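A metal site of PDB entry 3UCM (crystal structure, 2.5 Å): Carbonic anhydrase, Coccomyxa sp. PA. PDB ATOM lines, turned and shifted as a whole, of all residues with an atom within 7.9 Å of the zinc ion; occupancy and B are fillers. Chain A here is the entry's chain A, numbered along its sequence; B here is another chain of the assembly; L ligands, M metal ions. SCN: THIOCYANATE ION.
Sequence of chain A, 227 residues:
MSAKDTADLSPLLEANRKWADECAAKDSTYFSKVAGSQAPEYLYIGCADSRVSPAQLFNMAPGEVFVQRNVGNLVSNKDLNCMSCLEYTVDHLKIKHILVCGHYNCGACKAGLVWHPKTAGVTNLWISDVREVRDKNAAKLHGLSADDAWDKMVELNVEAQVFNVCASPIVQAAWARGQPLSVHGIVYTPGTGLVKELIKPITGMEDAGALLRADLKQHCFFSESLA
The backbone NH of Gly 72 lies close to the side-chain sulfur of Cys 47 (3.3 Å).
The side-chain sulfur (SG) of Cys 47 lies close to the backbone NH (N) of Asp 49, 3.7 Å away.
OD2 of Asp 49 lies within hydrogen-bond range of NE2 of Gln 38 of chain B, 3.0 Å away.
The side-chain sulfur (SG) of Cys 106 sits close to the backbone NH (N) of Ala 108, at 3.7 Å.
The side-chain carboxylate of Asp 49 lies within salt-bridge range of the guanidinium group of Arg 51 (3.0 Å).
O of Cys 106 is in hydrogen-bond range of NE1 of Trp 150, at 2.9 Å.
Residues that only touch the zinc ion: Asp 49 (3.9 Å).
The zinc ion is bound by a nitrogen (N) of the ligand (2.0 Å), a ring nitrogen (NE2) of His 103 (2.1 Å), the side-chain sulfur of Cys 47 (2.3 Å) and the side-chain sulfur of Cys 106 (2.4 Å).
The zinc ion has four donor atoms within binding distance.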
ATOM      1  N   GLY A  46      13.719  -3.266 -22.802  1.00  0.00           N
ATOM      2  CA  GLY A  46      14.896  -4.090 -22.468  1.00  0.00           C
ATOM      3  C   GLY A  46      14.616  -5.150 -21.413  1.00  0.00           C
ATOM      4  O   GLY A  46      13.430  -5.367 -21.040  1.00  0.00           O
ATOM      5  N   CYS A  47      15.663  -5.820 -20.921  1.00  0.00           N
ATOM      6  CA  CYS A  47      15.448  -6.990 -20.040  1.00  0.00           C
ATOM      7  C   CYS A  47      15.386  -6.621 -18.584  1.00  0.00           C
ATOM      8  O   CYS A  47      16.111  -5.712 -18.128  1.00  0.00           O
ATOM      9  CB  CYS A  47      16.501  -8.098 -20.272  1.00  0.00           C
ATOM     10  SG  CYS A  47      16.059  -9.784 -19.575  1.00  0.00           S
ATOM     11  N   ALA A  48      14.501  -7.310 -17.852  1.00  0.00           N
ATOM     12  CA  ALA A  48      14.403  -7.162 -16.378  1.00  0.00           C
ATOM     13  C   ALA A  48      15.659  -7.628 -15.566  1.00  0.00           C
ATOM     14  O   ALA A  48      15.744  -7.367 -14.340  1.00  0.00           O
ATOM     15  CB  ALA A  48      13.245  -7.958 -15.860  1.00  0.00           C
ATOM     16  N   ASP A  49      16.626  -8.281 -16.235  1.00  0.00           N
ATOM     17  CA  ASP A  49      17.946  -8.631 -15.640  1.00  0.00           C
ATOM     18  C   ASP A  49      18.566  -7.493 -14.785  1.00  0.00           C
ATOM     19  O   ASP A  49      18.637  -6.323 -15.206  1.00  0.00           O
ATOM     20  CB  ASP A  49      18.916  -9.032 -16.748  1.00  0.00           C
ATOM     21  CG  ASP A  49      20.214  -9.718 -16.213  1.00  0.00           C
ATOM     22  OD1 ASP A  49      21.137  -8.997 -15.756  1.00  0.00           O
ATOM     23  OD2 ASP A  49      20.345 -10.972 -16.270  1.00  0.00           O
ATOM     24  N   SER A  50      19.039  -7.856 -13.606  1.00  0.00           N
ATOM     25  CA  SER A  50      19.632  -6.891 -12.683  1.00  0.00           C
ATOM     26  C   SER A  50      20.994  -6.328 -13.090  1.00  0.00           C
ATOM     27  O   SER A  50      21.471  -5.410 -12.448  1.00  0.00           O
ATOM     28  CB  SER A  50      19.702  -7.450 -11.253  1.00  0.00           C
ATOM     29  OG  SER A  50      20.655  -8.488 -11.155  1.00  0.00           O
ATOM     30  N   ARG A  51      21.625  -6.852 -14.145  1.00  0.00           N
ATOM     31  CA  ARG A  51      22.913  -6.287 -14.611  1.00  0.00           C
ATOM     32  C   ARG A  51      22.787  -5.221 -15.741  1.00  0.00           C
ATOM     33  O   ARG A  51      23.810  -4.721 -16.253  1.00  0.00           O
ATOM     34  CB  ARG A  51      23.887  -7.400 -15.022  1.00  0.00           C
ATOM     35  CG  ARG A  51      24.181  -8.435 -13.877  1.00  0.00           C
ATOM     36  CD  ARG A  51      24.675  -9.784 -14.402  1.00  0.00           C
ATOM     37  NE  ARG A  51      23.736 -10.447 -15.340  1.00  0.00           N
ATOM     38  CZ  ARG A  51      24.050 -11.462 -16.154  1.00  0.00           C
ATOM     39  NH1 ARG A  51      25.308 -11.935 -16.214  1.00  0.00           N
ATOM     40  NH2 ARG A  51      23.118 -12.018 -16.935  1.00  0.00           N
ATOM     41  N   VAL A  52      21.540  -4.897 -16.146  1.00  0.00           N
ATOM     42  CA  VAL A  52      21.324  -4.064 -17.371  1.00  0.00           C
ATOM     43  C   VAL A  52      20.383  -2.877 -17.093  1.00  0.00           C
ATOM     44  O   VAL A  52      19.133  -2.974 -17.344  1.00  0.00           O
ATOM     45  CB  VAL A  52      20.827  -4.906 -18.620  1.00  0.00           C
ATOM     46  CG1 VAL A  52      20.911  -4.094 -19.912  1.00  0.00           C
ATOM     47  CG2 VAL A  52      21.600  -6.218 -18.779  1.00  0.00           C
ATOM     48  N   ASN A  70      11.069  -6.199 -19.144  1.00  0.00           N
ATOM     49  CA  ASN A  70      10.414  -7.503 -18.957  1.00  0.00           C
ATOM     50  C   ASN A  70      11.388  -8.670 -19.201  1.00  0.00           C
ATOM     51  O   ASN A  70      12.490  -8.459 -19.777  1.00  0.00           O
ATOM     52  CB  ASN A  70       9.124  -7.582 -19.795  1.00  0.00           C
ATOM     53  CG  ASN A  70       9.397  -7.733 -21.254  1.00  0.00           C
ATOM     54  OD1 ASN A  70       9.928  -8.755 -21.664  1.00  0.00           O
ATOM     55  ND2 ASN A  70       9.010  -6.744 -22.083  1.00  0.00           N
ATOM     56  N   VAL A  71      11.019  -9.889 -18.760  1.00  0.00           N
ATOM     57  CA  VAL A  71      11.905 -11.065 -18.855  1.00  0.00           C
ATOM     58  C   VAL A  71      12.101 -11.440 -20.316  1.00  0.00           C
ATOM     59  O   VAL A  71      11.166 -11.986 -20.941  1.00  0.00           O
ATOM     60  CB  VAL A  71      11.354 -12.290 -18.032  1.00  0.00           C
ATOM     61  CG1 VAL A  71      12.111 -13.623 -18.375  1.00  0.00           C
ATOM     62  CG2 VAL A  71      11.374 -12.004 -16.558  1.00  0.00           C
ATOM     63  N   GLY A  72      13.287 -11.081 -20.871  1.00  0.00           N
ATOM     64  CA  GLY A  72      13.642 -11.350 -22.285  1.00  0.00           C
ATOM     65  C   GLY A  72      13.457 -10.197 -23.301  1.00  0.00           C
ATOM     66  O   GLY A  72      13.636 -10.382 -24.503  1.00  0.00           O
ATOM     67  N   ASN A  73      13.133  -9.012 -22.841  1.00  0.00           N
ATOM     68  CA  ASN A  73      12.908  -7.915 -23.761  1.00  0.00           C
ATOM     69  C   ASN A  73      11.979  -8.180 -24.912  1.00  0.00           C
ATOM     70  O   ASN A  73      12.276  -7.783 -26.045  1.00  0.00           O
ATOM     71  CB  ASN A  73      14.206  -7.201 -24.265  1.00  0.00           C
ATOM     72  CG  ASN A  73      15.270  -8.152 -24.742  1.00  0.00           C
ATOM     73  OD1 ASN A  73      15.996  -8.753 -23.941  1.00  0.00           O
ATOM     74  ND2 ASN A  73      15.365  -8.314 -26.055  1.00  0.00           N
ATOM     75  N   CYS A 101      16.651  -3.402 -26.919  1.00  0.00           N
ATOM     76  CA  CYS A 101      17.951  -3.839 -26.395  1.00  0.00           C
ATOM     77  C   CYS A 101      17.960  -5.271 -25.783  1.00  0.00           C
ATOM     78  O   CYS A 101      17.247  -5.522 -24.829  1.00  0.00           O
ATOM     79  CB  CYS A 101      18.492  -2.803 -25.371  1.00  0.00           C
ATOM     80  SG  CYS A 101      20.188  -3.071 -24.651  1.00  0.00           S
ATOM     81  N   GLY A 102      18.781  -6.169 -26.357  1.00  0.00           N
ATOM     82  CA  GLY A 102      19.091  -7.475 -25.774  1.00  0.00           C
ATOM     83  C   GLY A 102      20.426  -7.421 -25.020  1.00  0.00           C
ATOM     84  O   GLY A 102      21.136  -6.383 -25.099  1.00  0.00           O
ATOM     85  N   HIS A 103      20.760  -8.504 -24.280  1.00  0.00           N
ATOM     86  CA  HIS A 103      22.045  -8.662 -23.527  1.00  0.00           C
ATOM     87  C   HIS A 103      22.662 -10.087 -23.578  1.00  0.00           C
ATOM     88  O   HIS A 103      21.924 -11.095 -23.557  1.00  0.00           O
ATOM     89  CB  HIS A 103      21.952  -8.182 -22.065  1.00  0.00           C
ATOM     90  CG  HIS A 103      21.167  -9.104 -21.165  1.00  0.00           C
ATOM     91  ND1 HIS A 103      21.755 -10.014 -20.323  1.00  0.00           N
ATOM     92  CD2 HIS A 103      19.822  -9.207 -20.942  1.00  0.00           C
ATOM     93  CE1 HIS A 103      20.826 -10.648 -19.630  1.00  0.00           C
ATOM     94  NE2 HIS A 103      19.642 -10.174 -19.976  1.00  0.00           N
ATOM     95  N   TYR A 104      23.990 -10.184 -23.650  1.00  0.00           N
ATOM     96  CA  TYR A 104      24.650 -11.475 -23.642  1.00  0.00           C
ATOM     97  C   TYR A 104      24.496 -12.024 -22.240  1.00  0.00           C
ATOM     98  O   TYR A 104      24.265 -11.252 -21.301  1.00  0.00           O
ATOM     99  CB  TYR A 104      26.106 -11.329 -24.043  1.00  0.00           C
ATOM    100  CG  TYR A 104      26.252 -10.993 -25.521  1.00  0.00           C
ATOM    101  CD1 TYR A 104      26.826  -9.789 -25.954  1.00  0.00           C
ATOM    102  CD2 TYR A 104      25.789 -11.901 -26.498  1.00  0.00           C
ATOM    103  CE1 TYR A 104      26.960  -9.504 -27.343  1.00  0.00           C
ATOM    104  CE2 TYR A 104      25.936 -11.648 -27.863  1.00  0.00           C
ATOM    105  CZ  TYR A 104      26.498 -10.434 -28.277  1.00  0.00           C
ATOM    106  OH  TYR A 104      26.546 -10.216 -29.622  1.00  0.00           O
ATOM    107  N   ASN A 105      24.569 -13.339 -22.097  1.00  0.00           N
ATOM    108  CA  ASN A 105      24.378 -14.015 -20.812  1.00  0.00           C
ATOM    109  C   ASN A 105      22.940 -13.862 -20.273  1.00  0.00           C
ATOM    110  O   ASN A 105      22.707 -13.807 -19.044  1.00  0.00           O
ATOM    111  CB  ASN A 105      25.440 -13.561 -19.800  1.00  0.00           C
ATOM    112  CG  ASN A 105      25.569 -14.520 -18.588  1.00  0.00           C
ATOM    113  OD1 ASN A 105      25.372 -14.108 -17.442  1.00  0.00           O
ATOM    114  ND2 ASN A 105      25.911 -15.797 -18.843  1.00  0.00           N
ATOM    115  N   CYS A 106      21.972 -13.775 -21.196  1.00  0.00           N
ATOM    116  CA  CYS A 106      20.575 -13.606 -20.784  1.00  0.00           C
ATOM    117  C   CYS A 106      19.881 -14.967 -20.502  1.00  0.00           C
ATOM    118  O   CYS A 106      19.707 -15.775 -21.423  1.00  0.00           O
ATOM    119  CB  CYS A 106      19.817 -12.798 -21.876  1.00  0.00           C
ATOM    120  SG  CYS A 106      17.939 -12.664 -21.705  1.00  0.00           S
ATOM    121  N   GLY A 107      19.465 -15.213 -19.260  1.00  0.00           N
ATOM    122  CA  GLY A 107      18.841 -16.476 -18.905  1.00  0.00           C
ATOM    123  C   GLY A 107      17.399 -16.703 -19.333  1.00  0.00           C
ATOM    124  O   GLY A 107      16.873 -17.790 -19.055  1.00  0.00           O
ATOM    125  N   ALA A 108      16.748 -15.684 -19.964  1.00  0.00           N
ATOM    126  CA  ALA A 108      15.400 -15.860 -20.575  1.00  0.00           C
ATOM    127  C   ALA A 108      15.559 -16.528 -21.964  1.00  0.00           C
ATOM    128  O   ALA A 108      14.732 -17.323 -22.398  1.00  0.00           O
ATOM    129  CB  ALA A 108      14.643 -14.489 -20.724  1.00  0.00           C
ATOM    130  N   CYS A 109      16.647 -16.172 -22.622  1.00  0.00           N
ATOM    131  CA  CYS A 109      17.066 -16.789 -23.843  1.00  0.00           C
ATOM    132  C   CYS A 109      17.669 -18.229 -23.618  1.00  0.00           C
ATOM    133  O   CYS A 109      17.471 -19.144 -24.458  1.00  0.00           O
ATOM    134  CB  CYS A 109      18.051 -15.852 -24.579  1.00  0.00           C
ATOM    135  SG  CYS A 109      17.328 -14.270 -25.266  1.00  0.00           S
ATOM    136  N   LYS A 110      18.370 -18.447 -22.502  1.00  0.00           N
ATOM    137  CA  LYS A 110      18.772 -19.809 -22.146  1.00  0.00           C
ATOM    138  C   LYS A 110      17.547 -20.707 -21.973  1.00  0.00           C
ATOM    139  O   LYS A 110      17.422 -21.688 -22.692  1.00  0.00           O
ATOM    140  CB  LYS A 110      19.616 -19.854 -20.857  1.00  0.00           C
ATOM    141  CG  LYS A 110      20.829 -20.744 -21.027  1.00  0.00           C
ATOM    142  CD  LYS A 110      21.078 -21.553 -19.798  1.00  0.00           C
ATOM    143  CE  LYS A 110      22.403 -22.336 -19.993  1.00  0.00           C
ATOM    144  NZ  LYS A 110      23.184 -22.495 -18.702  1.00  0.00           N
ATOM    145  N   TRP A 150      23.860 -19.712 -27.419  1.00  0.00           N
ATOM    146  CA  TRP A 150      23.325 -18.729 -26.503  1.00  0.00           C
ATOM    147  C   TRP A 150      23.538 -17.284 -27.040  1.00  0.00           C
ATOM    148  O   TRP A 150      22.546 -16.480 -27.085  1.00  0.00           O
ATOM    149  CB  TRP A 150      23.958 -18.969 -25.128  1.00  0.00           C
ATOM    150  CG  TRP A 150      23.329 -18.298 -23.958  1.00  0.00           C
ATOM    151  CD1 TRP A 150      22.229 -17.453 -23.951  1.00  0.00           C
ATOM    152  CD2 TRP A 150      23.787 -18.351 -22.585  1.00  0.00           C
ATOM    153  NE1 TRP A 150      21.966 -17.009 -22.675  1.00  0.00           N
ATOM    154  CE2 TRP A 150      22.898 -17.540 -21.815  1.00  0.00           C
ATOM    155  CE3 TRP A 150      24.853 -19.012 -21.939  1.00  0.00           C
ATOM    156  CZ2 TRP A 150      23.048 -17.384 -20.415  1.00  0.00           C
ATOM    157  CZ3 TRP A 150      25.011 -18.854 -20.566  1.00  0.00           C
ATOM    158  CH2 TRP A 150      24.104 -18.047 -19.817  1.00  0.00           C
ATOM    159  N   VAL A 154      20.412 -14.590 -28.478  1.00  0.00           N
ATOM    160  CA  VAL A 154      20.261 -13.213 -28.049  1.00  0.00           C
ATOM    161  C   VAL A 154      20.139 -12.264 -29.267  1.00  0.00           C
ATOM    162  O   VAL A 154      19.281 -11.377 -29.296  1.00  0.00           O
ATOM    163  CB  VAL A 154      21.434 -12.823 -27.097  1.00  0.00           C
ATOM    164  CG1 VAL A 154      21.589 -11.335 -26.999  1.00  0.00           C
ATOM    165  CG2 VAL A 154      21.244 -13.463 -25.713  1.00  0.00           C
ATOM    166  N   GLN B  38      23.924 -13.598 -11.959  1.00  0.00           N
ATOM    167  CA  GLN B  38      23.338 -12.531 -11.178  1.00  0.00           C
ATOM    168  C   GLN B  38      22.792 -13.226  -9.902  1.00  0.00           C
ATOM    169  O   GLN B  38      22.348 -14.387  -9.975  1.00  0.00           O
ATOM    170  CB  GLN B  38      22.220 -11.798 -11.974  1.00  0.00           C
ATOM    171  CG  GLN B  38      20.909 -12.566 -12.106  1.00  0.00           C
ATOM    172  CD  GLN B  38      19.796 -11.832 -12.878  1.00  0.00           C
ATOM    173  OE1 GLN B  38      19.383 -10.736 -12.532  1.00  0.00           O
ATOM    174  NE2 GLN B  38      19.266 -12.511 -13.896  1.00  0.00           N
ATOM    175  N   PHE B  66      16.746  -6.313  -9.616  1.00  0.00           N
ATOM    176  CA  PHE B  66      15.932  -6.836 -10.743  1.00  0.00           C
ATOM    177  C   PHE B  66      14.646  -5.972 -10.938  1.00  0.00           C
ATOM    178  O   PHE B  66      13.966  -5.659  -9.971  1.00  0.00           O
ATOM    179  CB  PHE B  66      15.585  -8.298 -10.409  1.00  0.00           C
ATOM    180  CG  PHE B  66      15.069  -9.133 -11.574  1.00  0.00           C
ATOM    181  CD1 PHE B  66      15.934  -9.890 -12.333  1.00  0.00           C
ATOM    182  CD2 PHE B  66      13.693  -9.216 -11.839  1.00  0.00           C
ATOM    183  CE1 PHE B  66      15.450 -10.725 -13.362  1.00  0.00           C
ATOM    184  CE2 PHE B  66      13.205 -10.040 -12.877  1.00  0.00           C
ATOM    185  CZ  PHE B  66      14.092 -10.798 -13.636  1.00  0.00           C
ATOM    186  N   TYR B  88      10.132 -15.438 -11.232  1.00  0.00           N
ATOM    187  CA  TYR B  88      11.566 -15.712 -11.492  1.00  0.00           C
ATOM    188  C   TYR B  88      12.461 -15.284 -10.362  1.00  0.00           C
ATOM    189  O   TYR B  88      13.484 -15.905 -10.081  1.00  0.00           O
ATOM    190  CB  TYR B  88      12.047 -15.043 -12.781  1.00  0.00           C
ATOM    191  CG  TYR B  88      13.413 -15.556 -13.270  1.00  0.00           C
ATOM    192  CD1 TYR B  88      13.530 -16.762 -13.963  1.00  0.00           C
ATOM    193  CD2 TYR B  88      14.574 -14.857 -12.988  1.00  0.00           C
ATOM    194  CE1 TYR B  88      14.756 -17.210 -14.415  1.00  0.00           C
ATOM    195  CE2 TYR B  88      15.797 -15.301 -13.419  1.00  0.00           C
ATOM    196  CZ  TYR B  88      15.893 -16.446 -14.144  1.00  0.00           C
ATOM    197  OH  TYR B  88      17.158 -16.863 -14.560  1.00  0.00           O
HETATM  198  S   SCN L   1      16.361 -13.643 -16.033  1.00  0.00           S
HETATM  199  C   SCN L   1      17.153 -12.888 -17.408  1.00  0.00           C
HETATM  200  N   SCN L   1      17.669 -12.386 -18.299  1.00  0.00           N
HETATM  201 ZN    ZN M   1      17.854 -11.208 -19.861  1.00  0.00          ZN
